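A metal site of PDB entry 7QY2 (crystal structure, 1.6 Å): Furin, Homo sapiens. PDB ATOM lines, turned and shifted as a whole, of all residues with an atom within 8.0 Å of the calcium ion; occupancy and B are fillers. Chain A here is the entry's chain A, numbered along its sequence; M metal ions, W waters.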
ATOM      1  N   GLY A 148      34.040 -12.637  25.563  1.00  0.00           N
ATOM      2  CA  GLY A 148      34.928 -13.622  25.004  1.00  0.00           C
ATOM      3  C   GLY A 148      34.940 -13.558  23.492  1.00  0.00           C
ATOM      4  O   GLY A 148      34.741 -12.492  22.892  1.00  0.00           O
ATOM      5  N   PRO A 149      35.180 -14.699  22.835  1.00  0.00           N
ATOM      6  CA  PRO A 149      35.100 -14.736  21.378  1.00  0.00           C
ATOM      7  C   PRO A 149      33.736 -14.290  20.898  1.00  0.00           C
ATOM      8  O   PRO A 149      32.746 -14.346  21.623  1.00  0.00           O
ATOM      9  CB  PRO A 149      35.362 -16.204  21.014  1.00  0.00           C
ATOM     10  CG  PRO A 149      35.832 -16.843  22.241  1.00  0.00           C
ATOM     11  CD  PRO A 149      35.382 -16.041  23.416  1.00  0.00           C
ATOM     12  N   GLU A 150      33.679 -13.888  19.630  1.00  0.00           N
ATOM     13  CA  GLU A 150      32.456 -13.351  19.047  1.00  0.00           C
ATOM     14  C   GLU A 150      31.283 -14.290  19.288  1.00  0.00           C
ATOM     15  O   GLU A 150      31.369 -15.488  19.050  1.00  0.00           O
ATOM     16  CB  GLU A 150      32.649 -13.132  17.545  1.00  0.00           C
ATOM     17  CG  GLU A 150      31.598 -12.239  16.931  1.00  0.00           C
ATOM     18  CD  GLU A 150      31.785 -10.784  17.329  1.00  0.00           C
ATOM     19  OE1 GLU A 150      32.947 -10.348  17.445  1.00  0.00           O
ATOM     20  OE2 GLU A 150      30.775 -10.086  17.539  1.00  0.00           O
ATOM     21  N   ASP A 151      30.185 -13.712  19.767  1.00  0.00           N
ATOM     22  CA  ASP A 151      28.942 -14.451  19.976  1.00  0.00           C
ATOM     23  C   ASP A 151      28.097 -14.445  18.707  1.00  0.00           C
ATOM     24  O   ASP A 151      26.900 -14.151  18.728  1.00  0.00           O
ATOM     25  CB  ASP A 151      28.168 -13.857  21.143  1.00  0.00           C
ATOM     26  CG  ASP A 151      28.764 -14.208  22.503  1.00  0.00           C
ATOM     27  OD1 ASP A 151      29.466 -15.242  22.614  1.00  0.00           O
ATOM     28  OD2 ASP A 151      28.507 -13.474  23.478  1.00  0.00           O
ATOM     29  N   ASP A 152      28.716 -14.767  17.566  1.00  0.00           N
ATOM     30  CA  ASP A 152      28.009 -14.750  16.286  1.00  0.00           C
ATOM     31  C   ASP A 152      27.421 -16.103  15.931  1.00  0.00           C
ATOM     32  O   ASP A 152      26.763 -16.229  14.891  1.00  0.00           O
ATOM     33  CB  ASP A 152      28.935 -14.250  15.165  1.00  0.00           C
ATOM     34  CG  ASP A 152      30.214 -15.063  15.013  1.00  0.00           C
ATOM     35  OD1 ASP A 152      30.378 -16.113  15.679  1.00  0.00           O
ATOM     36  OD2 ASP A 152      31.074 -14.634  14.201  1.00  0.00           O
ATOM     37  N   GLY A 153      27.578 -17.111  16.786  1.00  0.00           N
ATOM     38  CA  GLY A 153      27.048 -18.424  16.502  1.00  0.00           C
ATOM     39  C   GLY A 153      27.801 -19.191  15.446  1.00  0.00           C
ATOM     40  O   GLY A 153      27.299 -20.216  14.968  1.00  0.00           O
ATOM     41  N   LYS A 154      28.980 -18.724  15.054  1.00  0.00           N
ATOM     42  CA  LYS A 154      29.789 -19.454  14.102  1.00  0.00           C
ATOM     43  C   LYS A 154      31.260 -19.523  14.475  1.00  0.00           C
ATOM     44  O   LYS A 154      32.047 -20.087  13.698  1.00  0.00           O
ATOM     45  CB  LYS A 154      29.642 -18.855  12.696  1.00  0.00           C
ATOM     46  CG  LYS A 154      29.927 -17.370  12.563  1.00  0.00           C
ATOM     47  CD  LYS A 154      29.569 -16.937  11.145  1.00  0.00           C
ATOM     48  CE  LYS A 154      29.702 -15.442  10.956  1.00  0.00           C
ATOM     49  N   THR A 155      31.656 -19.019  15.618  1.00  0.00           N
ATOM     50  CA  THR A 155      33.046 -18.993  16.045  1.00  0.00           C
ATOM     51  C   THR A 155      33.319 -20.145  17.014  1.00  0.00           C
ATOM     52  O   THR A 155      32.485 -20.469  17.866  1.00  0.00           O
ATOM     53  CB  THR A 155      33.363 -17.651  16.710  1.00  0.00           C
ATOM     54  OG1 THR A 155      33.119 -16.596  15.755  1.00  0.00           O
ATOM     55  CG2 THR A 155      34.795 -17.589  17.170  1.00  0.00           C
ATOM     56  N   ALA A 185      30.918 -14.923  32.149  1.00  0.00           N
ATOM     57  CA  ALA A 185      29.607 -14.942  31.537  1.00  0.00           C
ATOM     58  C   ALA A 185      29.577 -15.972  30.410  1.00  0.00           C
ATOM     59  O   ALA A 185      30.496 -16.012  29.586  1.00  0.00           O
ATOM     60  CB  ALA A 185      29.265 -13.558  30.976  1.00  0.00           C
ATOM     61  N   SER A 186      28.535 -16.805  30.373  1.00  0.00           N
ATOM     62  CA  SER A 186      28.485 -17.870  29.372  1.00  0.00           C
ATOM     63  C   SER A 186      28.164 -17.369  27.970  1.00  0.00           C
ATOM     64  O   SER A 186      28.322 -18.131  27.007  1.00  0.00           O
ATOM     65  CB  SER A 186      27.459 -18.921  29.788  1.00  0.00           C
ATOM     66  OG  SER A 186      26.172 -18.354  29.869  1.00  0.00           O
ATOM     67  N   GLY A 187      27.716 -16.118  27.811  1.00  0.00           N
ATOM     68  CA  GLY A 187      27.591 -15.547  26.484  1.00  0.00           C
ATOM     69  C   GLY A 187      26.295 -14.816  26.192  1.00  0.00           C
ATOM     70  O   GLY A 187      25.290 -15.005  26.876  1.00  0.00           O
ATOM     71  N   ASN A 188      26.300 -13.983  25.137  1.00  0.00           N
ATOM     72  CA  ASN A 188      25.113 -13.247  24.724  1.00  0.00           C
ATOM     73  C   ASN A 188      24.596 -13.668  23.346  1.00  0.00           C
ATOM     74  O   ASN A 188      23.844 -12.918  22.719  1.00  0.00           O
ATOM     75  CB  ASN A 188      25.383 -11.740  24.687  1.00  0.00           C
ATOM     76  CG  ASN A 188      25.606 -11.142  26.065  1.00  0.00           C
ATOM     77  OD1 ASN A 188      24.883 -11.450  27.016  1.00  0.00           O
ATOM     78  ND2 ASN A 188      26.610 -10.283  26.168  1.00  0.00           N
ATOM     79  N   GLY A 189      24.995 -14.843  22.851  1.00  0.00           N
ATOM     80  CA  GLY A 189      24.719 -15.215  21.485  1.00  0.00           C
ATOM     81  C   GLY A 189      23.413 -15.956  21.215  1.00  0.00           C
ATOM     82  O   GLY A 189      23.264 -16.607  20.179  1.00  0.00           O
ATOM     83  N   GLY A 190      22.457 -15.826  22.128  1.00  0.00           N
ATOM     84  CA  GLY A 190      21.203 -16.564  21.998  1.00  0.00           C
ATOM     85  C   GLY A 190      20.496 -16.364  20.676  1.00  0.00           C
ATOM     86  O   GLY A 190      19.984 -17.324  20.087  1.00  0.00           O
ATOM     87  N   HIS A 193      21.694 -18.372  17.926  1.00  0.00           N
ATOM     88  CA  HIS A 193      21.700 -19.807  18.221  1.00  0.00           C
ATOM     89  C   HIS A 193      23.109 -20.284  18.571  1.00  0.00           C
ATOM     90  O   HIS A 193      23.501 -21.417  18.265  1.00  0.00           O
ATOM     91  CB  HIS A 193      21.106 -20.589  17.049  1.00  0.00           C
ATOM     92  CG  HIS A 193      19.776 -20.057  16.631  1.00  0.00           C
ATOM     93  ND1 HIS A 193      18.647 -20.180  17.411  1.00  0.00           N
ATOM     94  CD2 HIS A 193      19.399 -19.335  15.542  1.00  0.00           C
ATOM     95  CE1 HIS A 193      17.635 -19.583  16.820  1.00  0.00           C
ATOM     96  NE2 HIS A 193      18.059 -19.069  15.677  1.00  0.00           N
ATOM     97  N   ASP A 194      23.860 -19.431  19.251  1.00  0.00           N
ATOM     98  CA  ASP A 194      25.189 -19.826  19.716  1.00  0.00           C
ATOM     99  C   ASP A 194      25.063 -20.889  20.813  1.00  0.00           C
ATOM    100  O   ASP A 194      24.054 -20.974  21.526  1.00  0.00           O
ATOM    101  CB  ASP A 194      25.954 -18.606  20.222  1.00  0.00           C
ATOM    102  CG  ASP A 194      27.446 -18.809  20.188  1.00  0.00           C
ATOM    103  OD1 ASP A 194      27.933 -19.913  19.826  1.00  0.00           O
ATOM    104  OD2 ASP A 194      28.172 -17.832  20.536  1.00  0.00           O
ATOM    105  N   SER A 195      26.091 -21.723  20.910  1.00  0.00           N
ATOM    106  CA  SER A 195      26.161 -22.884  21.801  1.00  0.00           C
ATOM    107  C   SER A 195      27.481 -22.739  22.549  1.00  0.00           C
ATOM    108  O   SER A 195      28.547 -22.798  21.928  1.00  0.00           O
ATOM    109  CB  SER A 195      26.104 -24.174  20.972  1.00  0.00           C
ATOM    110  OG  SER A 195      25.930 -25.358  21.757  1.00  0.00           O
ATOM    111  N   CYS A 196      27.425 -22.501  23.864  1.00  0.00           N
ATOM    112  CA  CYS A 196      28.564 -21.830  24.492  1.00  0.00           C
ATOM    113  C   CYS A 196      29.755 -22.731  24.821  1.00  0.00           C
ATOM    114  O   CYS A 196      30.792 -22.208  25.253  1.00  0.00           O
ATOM    115  CB  CYS A 196      28.135 -21.089  25.772  1.00  0.00           C
ATOM    116  SG  CYS A 196      26.849 -21.768  26.865  1.00  0.00           S
ATOM    117  N   ASN A 197      29.689 -24.042  24.603  1.00  0.00           N
ATOM    118  CA  ASN A 197      30.933 -24.806  24.728  1.00  0.00           C
ATOM    119  C   ASN A 197      31.932 -24.461  23.617  1.00  0.00           C
ATOM    120  O   ASN A 197      33.103 -24.855  23.709  1.00  0.00           O
ATOM    121  CB  ASN A 197      30.684 -26.314  24.719  1.00  0.00           C
ATOM    122  CG  ASN A 197      29.992 -26.796  25.974  1.00  0.00           C
ATOM    123  OD1 ASN A 197      29.925 -26.087  26.983  1.00  0.00           O
ATOM    124  ND2 ASN A 197      29.481 -28.026  25.919  1.00  0.00           N
ATOM    125  N   CYS A 198      31.493 -23.754  22.577  1.00  0.00           N
ATOM    126  CA  CYS A 198      32.373 -23.274  21.523  1.00  0.00           C
ATOM    127  C   CYS A 198      33.180 -22.055  21.935  1.00  0.00           C
ATOM    128  O   CYS A 198      33.987 -21.561  21.137  1.00  0.00           O
ATOM    129  CB  CYS A 198      31.554 -22.959  20.279  1.00  0.00           C
ATOM    130  SG  CYS A 198      30.766 -24.391  19.530  1.00  0.00           S
ATOM    131  N   ASP A 199      32.963 -21.542  23.154  1.00  0.00           N
ATOM    132  CA  ASP A 199      33.689 -20.438  23.764  1.00  0.00           C
ATOM    133  C   ASP A 199      34.617 -21.065  24.806  1.00  0.00           C
ATOM    134  O   ASP A 199      34.134 -21.544  25.846  1.00  0.00           O
ATOM    135  CB  ASP A 199      32.688 -19.442  24.337  1.00  0.00           C
ATOM    136  CG  ASP A 199      33.294 -18.410  25.278  1.00  0.00           C
ATOM    137  OD1 ASP A 199      34.452 -18.527  25.722  1.00  0.00           O
ATOM    138  OD2 ASP A 199      32.553 -17.454  25.605  1.00  0.00           O
ATOM    139  N   GLY A 200      35.916 -21.104  24.503  1.00  0.00           N
ATOM    140  CA  GLY A 200      36.866 -21.831  25.339  1.00  0.00           C
ATOM    141  C   GLY A 200      37.126 -21.185  26.674  1.00  0.00           C
ATOM    142  O   GLY A 200      37.719 -21.836  27.554  1.00  0.00           O
ATOM    143  N   THR A 202      34.474 -19.707  28.716  1.00  0.00           N
ATOM    144  CA  THR A 202      33.430 -20.220  29.595  1.00  0.00           C
ATOM    145  C   THR A 202      33.462 -21.742  29.667  1.00  0.00           C
ATOM    146  O   THR A 202      33.124 -22.326  30.699  1.00  0.00           O
ATOM    147  CB  THR A 202      32.066 -19.679  29.144  1.00  0.00           C
ATOM    148  OG1 THR A 202      31.100 -19.890  30.174  1.00  0.00           O
ATOM    149  CG2 THR A 202      31.601 -20.308  27.843  1.00  0.00           C
ATOM    150  N   TYR A 222      18.917 -13.626  24.863  1.00  0.00           N
ATOM    151  CA  TYR A 222      20.342 -13.618  24.574  1.00  0.00           C
ATOM    152  C   TYR A 222      21.087 -14.808  25.159  1.00  0.00           C
ATOM    153  O   TYR A 222      22.292 -14.959  24.897  1.00  0.00           O
ATOM    154  CB  TYR A 222      20.957 -12.305  25.084  1.00  0.00           C
ATOM    155  CG  TYR A 222      20.614 -12.032  26.525  1.00  0.00           C
ATOM    156  CD1 TYR A 222      21.259 -12.713  27.548  1.00  0.00           C
ATOM    157  CD2 TYR A 222      19.628 -11.106  26.884  1.00  0.00           C
ATOM    158  CE1 TYR A 222      20.947 -12.496  28.860  1.00  0.00           C
ATOM    159  CE2 TYR A 222      19.310 -10.882  28.206  1.00  0.00           C
ATOM    160  CZ  TYR A 222      19.978 -11.584  29.190  1.00  0.00           C
ATOM    161  OH  TYR A 222      19.700 -11.388  30.522  1.00  0.00           O
ATOM    162  N   GLU A 224      22.836 -18.333  25.916  1.00  0.00           N
ATOM    163  CA  GLU A 224      23.384 -19.518  25.247  1.00  0.00           C
ATOM    164  C   GLU A 224      23.301 -20.707  26.195  1.00  0.00           C
ATOM    165  O   GLU A 224      23.674 -20.599  27.374  1.00  0.00           O
ATOM    166  CB  GLU A 224      24.842 -19.297  24.815  1.00  0.00           C
ATOM    167  CG  GLU A 224      25.058 -18.111  23.883  1.00  0.00           C
ATOM    168  CD  GLU A 224      26.511 -17.917  23.509  1.00  0.00           C
ATOM    169  OE1 GLU A 224      27.229 -18.930  23.304  1.00  0.00           O
ATOM    170  OE2 GLU A 224      26.946 -16.741  23.416  1.00  0.00           O
ATOM    171  N   CYS A 226      24.646 -24.433  27.274  1.00  0.00           N
ATOM    172  CA  CYS A 226      25.730 -25.394  27.085  1.00  0.00           C
ATOM    173  C   CYS A 226      25.976 -26.143  28.391  1.00  0.00           C
ATOM    174  O   CYS A 226      25.528 -25.732  29.461  1.00  0.00           O
ATOM    175  CB  CYS A 226      27.020 -24.731  26.597  1.00  0.00           C
ATOM    176  SG  CYS A 226      27.690 -23.434  27.646  1.00  0.00           S
ATOM    177  N   ARG A 412      24.284 -25.303  15.223  1.00  0.00           N
ATOM    178  CA  ARG A 412      24.550 -23.868  15.094  1.00  0.00           C
ATOM    179  C   ARG A 412      24.311 -23.515  13.629  1.00  0.00           C
ATOM    180  O   ARG A 412      25.214 -23.679  12.787  1.00  0.00           O
ATOM    181  CB  ARG A 412      25.961 -23.525  15.556  1.00  0.00           C
ATOM    182  CG  ARG A 412      26.130 -23.596  17.080  1.00  0.00           C
ATOM    183  CD  ARG A 412      27.255 -22.711  17.592  1.00  0.00           C
ATOM    184  NE  ARG A 412      28.503 -22.941  16.855  1.00  0.00           N
ATOM    185  CZ  ARG A 412      29.575 -22.174  16.956  1.00  0.00           C
ATOM    186  NH1 ARG A 412      29.577 -21.131  17.771  1.00  0.00           N
ATOM    187  NH2 ARG A 412      30.659 -22.458  16.244  1.00  0.00           N
HETATM  188 CA    CA M   1      29.159 -17.555  22.637  1.00  0.00          CA
HETATM  189  O   HOH W   1      31.399 -17.123  21.745  1.00  0.00           O
HETATM  190  O   HOH W   2      30.062 -19.746  21.878  1.00  0.00           O
HETATM  191  O   HOH W   3      29.965 -17.791  24.834  1.00  0.00           O
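N of Asn 188 is in hydrogen-bond range of OD2 of Asp 151 (2.8 Å). The backbone NH (N) of Asp 194 sits at hydrogen-bond distance from the backbone carbonyl oxygen (O) of Gly 189. The side-chain carboxylate (OD1) of Asp 194 lies within salt-bridge range of the guanidinium group (NH1) of Arg 412. N of Gly 189 sits close to OE2 of Glu 224. N of Asn 188 lies close to OE2 of Glu 224 (3.3 Å). SG of Cys 196 forms a disulfide with SG of Cys 226 (2.0 Å).
Of the 27 residues printed, 3 come within 4 Å of the calcium ion.
OD1 of Asp 151 binds the calcium ion, at 2.3 Å. The calcium ion is bound by the side-chain carboxylate (OD2) of Asp 194, at 2.3 Å. The calcium ion is bound by water W3 (2.4 Å). Water W1 is bound to the calcium ion, at 2.4 Å. OE1 of Glu 224 binds the calcium ion, at 2.5 Å. The calcium ion is bound by OE2 of Glu 224 (2.5 Å). Water W2 is bound to the calcium ion (2.5 Å). The calcium ion has seven donor atoms within binding distance.
Water W3 bridges OD2 of Asp 199 (2.7 Å) and O of Ser 186 (2.7 Å). Water W2 bridges OD1 of Asp 194 (3.0 Å) and O of Ser 195 (3.4 Å).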
